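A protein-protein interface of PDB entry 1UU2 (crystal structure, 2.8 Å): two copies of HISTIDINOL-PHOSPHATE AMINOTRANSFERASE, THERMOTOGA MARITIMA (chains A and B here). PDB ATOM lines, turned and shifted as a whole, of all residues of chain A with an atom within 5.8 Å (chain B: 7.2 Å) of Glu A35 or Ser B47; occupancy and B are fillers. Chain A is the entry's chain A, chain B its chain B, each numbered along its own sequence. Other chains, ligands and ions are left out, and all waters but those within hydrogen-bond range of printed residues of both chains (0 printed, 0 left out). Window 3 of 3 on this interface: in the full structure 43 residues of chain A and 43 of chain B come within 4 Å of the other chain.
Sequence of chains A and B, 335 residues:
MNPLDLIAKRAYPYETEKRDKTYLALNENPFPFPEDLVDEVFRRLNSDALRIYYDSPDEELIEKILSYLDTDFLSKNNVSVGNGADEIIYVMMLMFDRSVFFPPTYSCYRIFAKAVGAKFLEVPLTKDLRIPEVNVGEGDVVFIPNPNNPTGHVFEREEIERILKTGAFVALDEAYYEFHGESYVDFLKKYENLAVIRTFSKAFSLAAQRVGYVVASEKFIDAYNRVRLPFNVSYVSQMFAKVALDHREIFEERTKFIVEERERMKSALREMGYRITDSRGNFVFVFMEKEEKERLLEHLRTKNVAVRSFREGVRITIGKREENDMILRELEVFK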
ATOM      1  N   PHE A  31      18.561 -10.454  12.240  1.00  0.00           N
ATOM      2  CA  PHE A  31      19.482  -9.393  11.837  1.00  0.00           C
ATOM      3  C   PHE A  31      18.804  -8.068  11.542  1.00  0.00           C
ATOM      4  O   PHE A  31      17.663  -8.027  11.078  1.00  0.00           O
ATOM      5  CB  PHE A  31      20.273  -9.808  10.604  1.00  0.00           C
ATOM      6  CG  PHE A  31      20.718 -11.231  10.627  1.00  0.00           C
ATOM      7  CD1 PHE A  31      19.932 -12.221  10.049  1.00  0.00           C
ATOM      8  CD2 PHE A  31      21.920 -11.586  11.229  1.00  0.00           C
ATOM      9  CE1 PHE A  31      20.341 -13.548  10.066  1.00  0.00           C
ATOM     10  CE2 PHE A  31      22.338 -12.908  11.253  1.00  0.00           C
ATOM     11  CZ  PHE A  31      21.546 -13.893  10.669  1.00  0.00           C
ATOM     12  N   PRO A  32      19.513  -6.959  11.794  1.00  0.00           N
ATOM     13  CA  PRO A  32      18.968  -5.625  11.550  1.00  0.00           C
ATOM     14  C   PRO A  32      18.843  -5.378  10.055  1.00  0.00           C
ATOM     15  O   PRO A  32      19.469  -6.067   9.251  1.00  0.00           O
ATOM     16  CB  PRO A  32      19.997  -4.717  12.205  1.00  0.00           C
ATOM     17  CG  PRO A  32      21.267  -5.449  11.966  1.00  0.00           C
ATOM     18  CD  PRO A  32      20.890  -6.873  12.301  1.00  0.00           C
ATOM     19  N   PHE A  33      18.029  -4.400   9.684  1.00  0.00           N
ATOM     20  CA  PHE A  33      17.843  -4.085   8.280  1.00  0.00           C
ATOM     21  C   PHE A  33      19.193  -3.712   7.693  1.00  0.00           C
ATOM     22  O   PHE A  33      19.948  -2.961   8.299  1.00  0.00           O
ATOM     23  CB  PHE A  33      16.871  -2.919   8.123  1.00  0.00           C
ATOM     24  CG  PHE A  33      16.422  -2.704   6.719  1.00  0.00           C
ATOM     25  CD1 PHE A  33      15.693  -3.683   6.057  1.00  0.00           C
ATOM     26  CD2 PHE A  33      16.759  -1.547   6.042  1.00  0.00           C
ATOM     27  CE1 PHE A  33      15.308  -3.513   4.736  1.00  0.00           C
ATOM     28  CE2 PHE A  33      16.381  -1.363   4.719  1.00  0.00           C
ATOM     29  CZ  PHE A  33      15.653  -2.352   4.063  1.00  0.00           C
ATOM     30  N   PRO A  34      19.520  -4.235   6.507  1.00  0.00           N
ATOM     31  CA  PRO A  34      20.806  -3.921   5.881  1.00  0.00           C
ATOM     32  C   PRO A  34      21.171  -2.442   5.992  1.00  0.00           C
ATOM     33  O   PRO A  34      20.517  -1.581   5.404  1.00  0.00           O
ATOM     34  CB  PRO A  34      20.601  -4.376   4.444  1.00  0.00           C
ATOM     35  CG  PRO A  34      19.734  -5.581   4.619  1.00  0.00           C
ATOM     36  CD  PRO A  34      18.714  -5.109   5.638  1.00  0.00           C
ATOM     37  N   GLU A  35      22.222  -2.172   6.761  1.00  0.00           N
ATOM     38  CA  GLU A  35      22.727  -0.819   7.001  1.00  0.00           C
ATOM     39  C   GLU A  35      22.691   0.052   5.746  1.00  0.00           C
ATOM     40  O   GLU A  35      22.012   1.082   5.697  1.00  0.00           O
ATOM     41  CB  GLU A  35      24.171  -0.896   7.508  1.00  0.00           C
ATOM     42  CG  GLU A  35      24.627   0.295   8.337  1.00  0.00           C
ATOM     43  CD  GLU A  35      24.166   0.203   9.779  1.00  0.00           C
ATOM     44  OE2 GLU A  35      23.394   1.080  10.222  1.00  0.00           O
ATOM     45  N   ASP A  36      23.446  -0.374   4.739  1.00  0.00           N
ATOM     46  CA  ASP A  36      23.544   0.328   3.467  1.00  0.00           C
ATOM     47  C   ASP A  36      22.169   0.620   2.896  1.00  0.00           C
ATOM     48  O   ASP A  36      21.916   1.718   2.405  1.00  0.00           O
ATOM     49  CB  ASP A  36      24.336  -0.521   2.478  1.00  0.00           C
ATOM     50  CG  ASP A  36      25.671  -0.966   3.043  1.00  0.00           C
ATOM     51  OD1 ASP A  36      26.610  -0.145   3.065  1.00  0.00           O
ATOM     52  OD2 ASP A  36      25.768  -2.130   3.488  1.00  0.00           O
ATOM     53  N   LEU A  37      21.279  -0.364   2.978  1.00  0.00           N
ATOM     54  CA  LEU A  37      19.932  -0.201   2.454  1.00  0.00           C
ATOM     55  C   LEU A  37      19.138   0.866   3.195  1.00  0.00           C
ATOM     56  O   LEU A  37      18.168   1.406   2.666  1.00  0.00           O
ATOM     57  CB  LEU A  37      19.191  -1.537   2.481  1.00  0.00           C
ATOM     58  CG  LEU A  37      19.827  -2.618   1.611  1.00  0.00           C
ATOM     59  CD1 LEU A  37      18.900  -3.820   1.553  1.00  0.00           C
ATOM     60  CD2 LEU A  37      20.090  -2.053   0.223  1.00  0.00           C
ATOM     61  N   VAL A  38      19.549   1.188   4.416  1.00  0.00           N
ATOM     62  CA  VAL A  38      18.870   2.225   5.173  1.00  0.00           C
ATOM     63  C   VAL A  38      19.266   3.550   4.547  1.00  0.00           C
ATOM     64  O   VAL A  38      18.430   4.424   4.337  1.00  0.00           O
ATOM     65  CB  VAL A  38      19.303   2.236   6.634  1.00  0.00           C
ATOM     66  CG1 VAL A  38      18.683   3.428   7.353  1.00  0.00           C
ATOM     67  CG2 VAL A  38      18.895   0.922   7.298  1.00  0.00           C
ATOM     68  N   ASP A  39      20.548   3.679   4.225  1.00  0.00           N
ATOM     69  CA  ASP A  39      21.045   4.900   3.616  1.00  0.00           C
ATOM     70  C   ASP A  39      20.556   5.065   2.186  1.00  0.00           C
ATOM     71  O   ASP A  39      20.807   6.087   1.553  1.00  0.00           O
ATOM     72  CB  ASP A  39      22.574   4.937   3.650  1.00  0.00           C
ATOM     73  N   GLU A  40      19.849   4.067   1.671  1.00  0.00           N
ATOM     74  CA  GLU A  40      19.323   4.169   0.320  1.00  0.00           C
ATOM     75  C   GLU A  40      17.881   4.629   0.350  1.00  0.00           C
ATOM     76  O   GLU A  40      17.430   5.289  -0.574  1.00  0.00           O
ATOM     77  CB  GLU A  40      19.421   2.833  -0.419  1.00  0.00           C
ATOM     78  CG  GLU A  40      18.630   2.763  -1.722  1.00  0.00           C
ATOM     79  CD  GLU A  40      19.036   3.825  -2.732  1.00  0.00           C
ATOM     80  OE1 GLU A  40      19.305   3.458  -3.893  1.00  0.00           O
ATOM     81  OE2 GLU A  40      19.075   5.017  -2.370  1.00  0.00           O
ATOM     82  N   ARG A 254      19.641 -14.530   4.064  1.00  0.00           N
ATOM     83  CA  ARG A 254      19.291 -14.584   5.477  1.00  0.00           C
ATOM     84  C   ARG A 254      18.253 -15.675   5.696  1.00  0.00           C
ATOM     85  O   ARG A 254      18.278 -16.379   6.701  1.00  0.00           O
ATOM     86  CB  ARG A 254      18.715 -13.246   5.942  1.00  0.00           C
ATOM     87  CG  ARG A 254      19.699 -12.094   5.944  1.00  0.00           C
ATOM     88  CD  ARG A 254      19.112 -10.905   6.683  1.00  0.00           C
ATOM     89  NE  ARG A 254      20.029  -9.772   6.724  1.00  0.00           N
ATOM     90  CZ  ARG A 254      19.793  -8.643   7.384  1.00  0.00           C
ATOM     91  NH1 ARG A 254      18.663  -8.498   8.064  1.00  0.00           N
ATOM     92  NH2 ARG A 254      20.685  -7.660   7.363  1.00  0.00           N
ATOM     93  N   PHE B  42      17.539   9.828  10.894  1.00  0.00           N
ATOM     94  CA  PHE B  42      18.279   8.574  10.949  1.00  0.00           C
ATOM     95  C   PHE B  42      19.649   8.712  11.586  1.00  0.00           C
ATOM     96  O   PHE B  42      20.324   7.715  11.820  1.00  0.00           O
ATOM     97  CB  PHE B  42      18.399   7.943   9.566  1.00  0.00           C
ATOM     98  CG  PHE B  42      19.202   8.747   8.598  1.00  0.00           C
ATOM     99  CD1 PHE B  42      20.582   8.848   8.731  1.00  0.00           C
ATOM    100  CD2 PHE B  42      18.578   9.390   7.550  1.00  0.00           C
ATOM    101  CE1 PHE B  42      21.327   9.589   7.818  1.00  0.00           C
ATOM    102  CE2 PHE B  42      19.314  10.130   6.636  1.00  0.00           C
ATOM    103  CZ  PHE B  42      20.691  10.229   6.770  1.00  0.00           C
ATOM    104  N   LEU B  45      18.226   7.073  14.093  1.00  0.00           N
ATOM    105  CA  LEU B  45      17.567   5.769  13.946  1.00  0.00           C
ATOM    106  C   LEU B  45      18.533   4.590  13.868  1.00  0.00           C
ATOM    107  O   LEU B  45      19.467   4.598  13.079  1.00  0.00           O
ATOM    108  CB  LEU B  45      16.668   5.756  12.705  1.00  0.00           C
ATOM    109  CG  LEU B  45      17.148   5.228  11.351  1.00  0.00           C
ATOM    110  CD1 LEU B  45      17.255   3.723  11.411  1.00  0.00           C
ATOM    111  CD2 LEU B  45      16.142   5.630  10.281  1.00  0.00           C
ATOM    112  N   ASN B  46      18.268   3.569  14.677  1.00  0.00           N
ATOM    113  CA  ASN B  46      19.099   2.367  14.727  1.00  0.00           C
ATOM    114  C   ASN B  46      18.619   1.323  13.725  1.00  0.00           C
ATOM    115  O   ASN B  46      17.461   0.912  13.745  1.00  0.00           O
ATOM    116  CB  ASN B  46      19.051   1.768  16.135  1.00  0.00           C
ATOM    117  CG  ASN B  46      19.908   0.510  16.278  1.00  0.00           C
ATOM    118  OD1 ASN B  46      20.443  -0.018  15.305  1.00  0.00           O
ATOM    119  ND2 ASN B  46      20.030   0.030  17.506  1.00  0.00           N
ATOM    120  N   SER B  47      19.524   0.886  12.857  1.00  0.00           N
ATOM    121  CA  SER B  47      19.198  -0.113  11.853  1.00  0.00           C
ATOM    122  C   SER B  47      18.851  -1.456  12.483  1.00  0.00           C
ATOM    123  O   SER B  47      18.389  -2.374  11.800  1.00  0.00           O
ATOM    124  CB  SER B  47      20.379  -0.291  10.905  1.00  0.00           C
ATOM    125  OG  SER B  47      20.141  -1.358  10.006  1.00  0.00           O
ATOM    126  N   ASP B  48      19.076  -1.568  13.788  1.00  0.00           N
ATOM    127  CA  ASP B  48      18.806  -2.804  14.513  1.00  0.00           C
ATOM    128  C   ASP B  48      17.401  -2.796  15.099  1.00  0.00           C
ATOM    129  O   ASP B  48      16.875  -3.839  15.490  1.00  0.00           O
ATOM    130  CB  ASP B  48      19.823  -2.980  15.642  1.00  0.00           C
ATOM    131  CG  ASP B  48      19.776  -4.361  16.258  1.00  0.00           C
ATOM    132  OD1 ASP B  48      20.199  -4.507  17.425  1.00  0.00           O
ATOM    133  OD2 ASP B  48      19.329  -5.304  15.569  1.00  0.00           O
ATOM    134  N   ALA B  49      16.799  -1.617  15.172  1.00  0.00           N
ATOM    135  CA  ALA B  49      15.459  -1.502  15.723  1.00  0.00           C
ATOM    136  C   ALA B  49      14.428  -1.854  14.664  1.00  0.00           C
ATOM    137  O   ALA B  49      13.378  -2.412  14.969  1.00  0.00           O
ATOM    138  CB  ALA B  49      15.217  -0.090  16.239  1.00  0.00           C
ATOM    139  N   LEU B  50      14.744  -1.539  13.415  1.00  0.00           N
ATOM    140  CA  LEU B  50      13.837  -1.796  12.303  1.00  0.00           C
ATOM    141  C   LEU B  50      13.291  -3.225  12.233  1.00  0.00           C
ATOM    142  O   LEU B  50      12.219  -3.454  11.672  1.00  0.00           O
ATOM    143  CB  LEU B  50      14.534  -1.457  10.978  1.00  0.00           C
ATOM    144  CG  LEU B  50      15.018  -0.018  10.759  1.00  0.00           C
ATOM    145  CD1 LEU B  50      15.745   0.076   9.429  1.00  0.00           C
ATOM    146  CD2 LEU B  50      13.842   0.943  10.791  1.00  0.00           C
ATOM    147  N   ARG B  51      14.013  -4.178  12.812  1.00  0.00           N
ATOM    148  CA  ARG B  51      13.595  -5.573  12.759  1.00  0.00           C
ATOM    149  C   ARG B  51      12.632  -6.038  13.844  1.00  0.00           C
ATOM    150  O   ARG B  51      11.921  -7.025  13.651  1.00  0.00           O
ATOM    151  CB  ARG B  51      14.823  -6.485  12.766  1.00  0.00           C
ATOM    152  CG  ARG B  51      15.730  -6.297  13.969  1.00  0.00           C
ATOM    153  CD  ARG B  51      16.852  -7.312  13.949  1.00  0.00           C
ATOM    154  NE  ARG B  51      16.651  -8.351  14.945  1.00  0.00           N
ATOM    155  CZ  ARG B  51      16.902  -8.190  16.236  1.00  0.00           C
ATOM    156  NH1 ARG B  51      17.369  -7.031  16.675  1.00  0.00           N
ATOM    157  NH2 ARG B  51      16.675  -9.180  17.087  1.00  0.00           N
ATOM    158  N   TYR B 235       8.415   2.903  13.303  1.00  0.00           N
ATOM    159  CA  TYR B 235       9.585   3.380  14.022  1.00  0.00           C
ATOM    160  C   TYR B 235      10.100   4.686  13.419  1.00  0.00           C
ATOM    161  O   TYR B 235      10.381   5.647  14.138  1.00  0.00           O
ATOM    162  CB  TYR B 235      10.663   2.294  13.972  1.00  0.00           C
ATOM    163  CG  TYR B 235      12.029   2.692  14.484  1.00  0.00           C
ATOM    164  CD1 TYR B 235      12.189   3.277  15.740  1.00  0.00           C
ATOM    165  CD2 TYR B 235      13.173   2.437  13.724  1.00  0.00           C
ATOM    166  CE1 TYR B 235      13.451   3.596  16.226  1.00  0.00           C
ATOM    167  CE2 TYR B 235      14.440   2.751  14.203  1.00  0.00           C
ATOM    168  CZ  TYR B 235      14.571   3.330  15.455  1.00  0.00           C
ATOM    169  OH  TYR B 235      15.820   3.634  15.935  1.00  0.00           O
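The backbone carbonyl oxygen of Phe A31 sits at hydrogen-bond distance from the guanidinium group of Arg A254 (3.2 Å).
The guanidinium group of Arg A254 sits at hydrogen-bond distance from the backbone carbonyl oxygen of Pro A32 (2.8 Å).
OD1 of Asn B46 lies within hydrogen-bond range of N of Asp B48 (2.6 Å).
The guanidinium group (NH1) of Arg B51 lies within salt-bridge range of the side-chain carboxylate (OD2) of Asp B48.
No position is printed for both chains.
Of the 9 printed residues of chain B, 4 touch a printed residue of chain A.
Hydrophobic or aromatic side chains of chain A that line the printed part of chain B: Pro A32, Phe A33 and Val A38.
Among the printed residues, pairs that only touch across the chains: Pro A32 with Ser B47 (2.9 Å), Phe A31 with Arg B51 (3.1 Å), Pro A32 with Asp B48 (3.2 Å), Glu A35 with Ser B47 (3.4 Å), Pro A32 with Arg B51 (3.4 Å), Phe A33 with Leu B50 (3.5 Å), Val A38 with Ser B47 (3.8 Å) and Val A38 with Leu B50 (3.9 Å).
The backbone NH (N) of Phe A33 sits at hydrogen-bond distance from the backbone carbonyl oxygen (O) of Ser B47, at 3.0 Å.
Glu A35 touches just one residue of chain B: Ser B47 (3.4 Å).
Of chain A, only Pro A32, Phe A33, Glu A35 and Val A38 come within 4 Å of Ser B47.
Of the printed residues of chain B, Phe A33 touches Ser B47 and Leu B50.
Of the printed residues of chain A, Arg B51 touches Phe A31 and Pro A32.
Of the printed residues of chain B, Phe A31 touches Arg B51.
Ala B49 touches none of the printed residues of chain A.
The nearest residue of chain A that does not touch Ser B47 is Pro A34 (4.3 Å).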
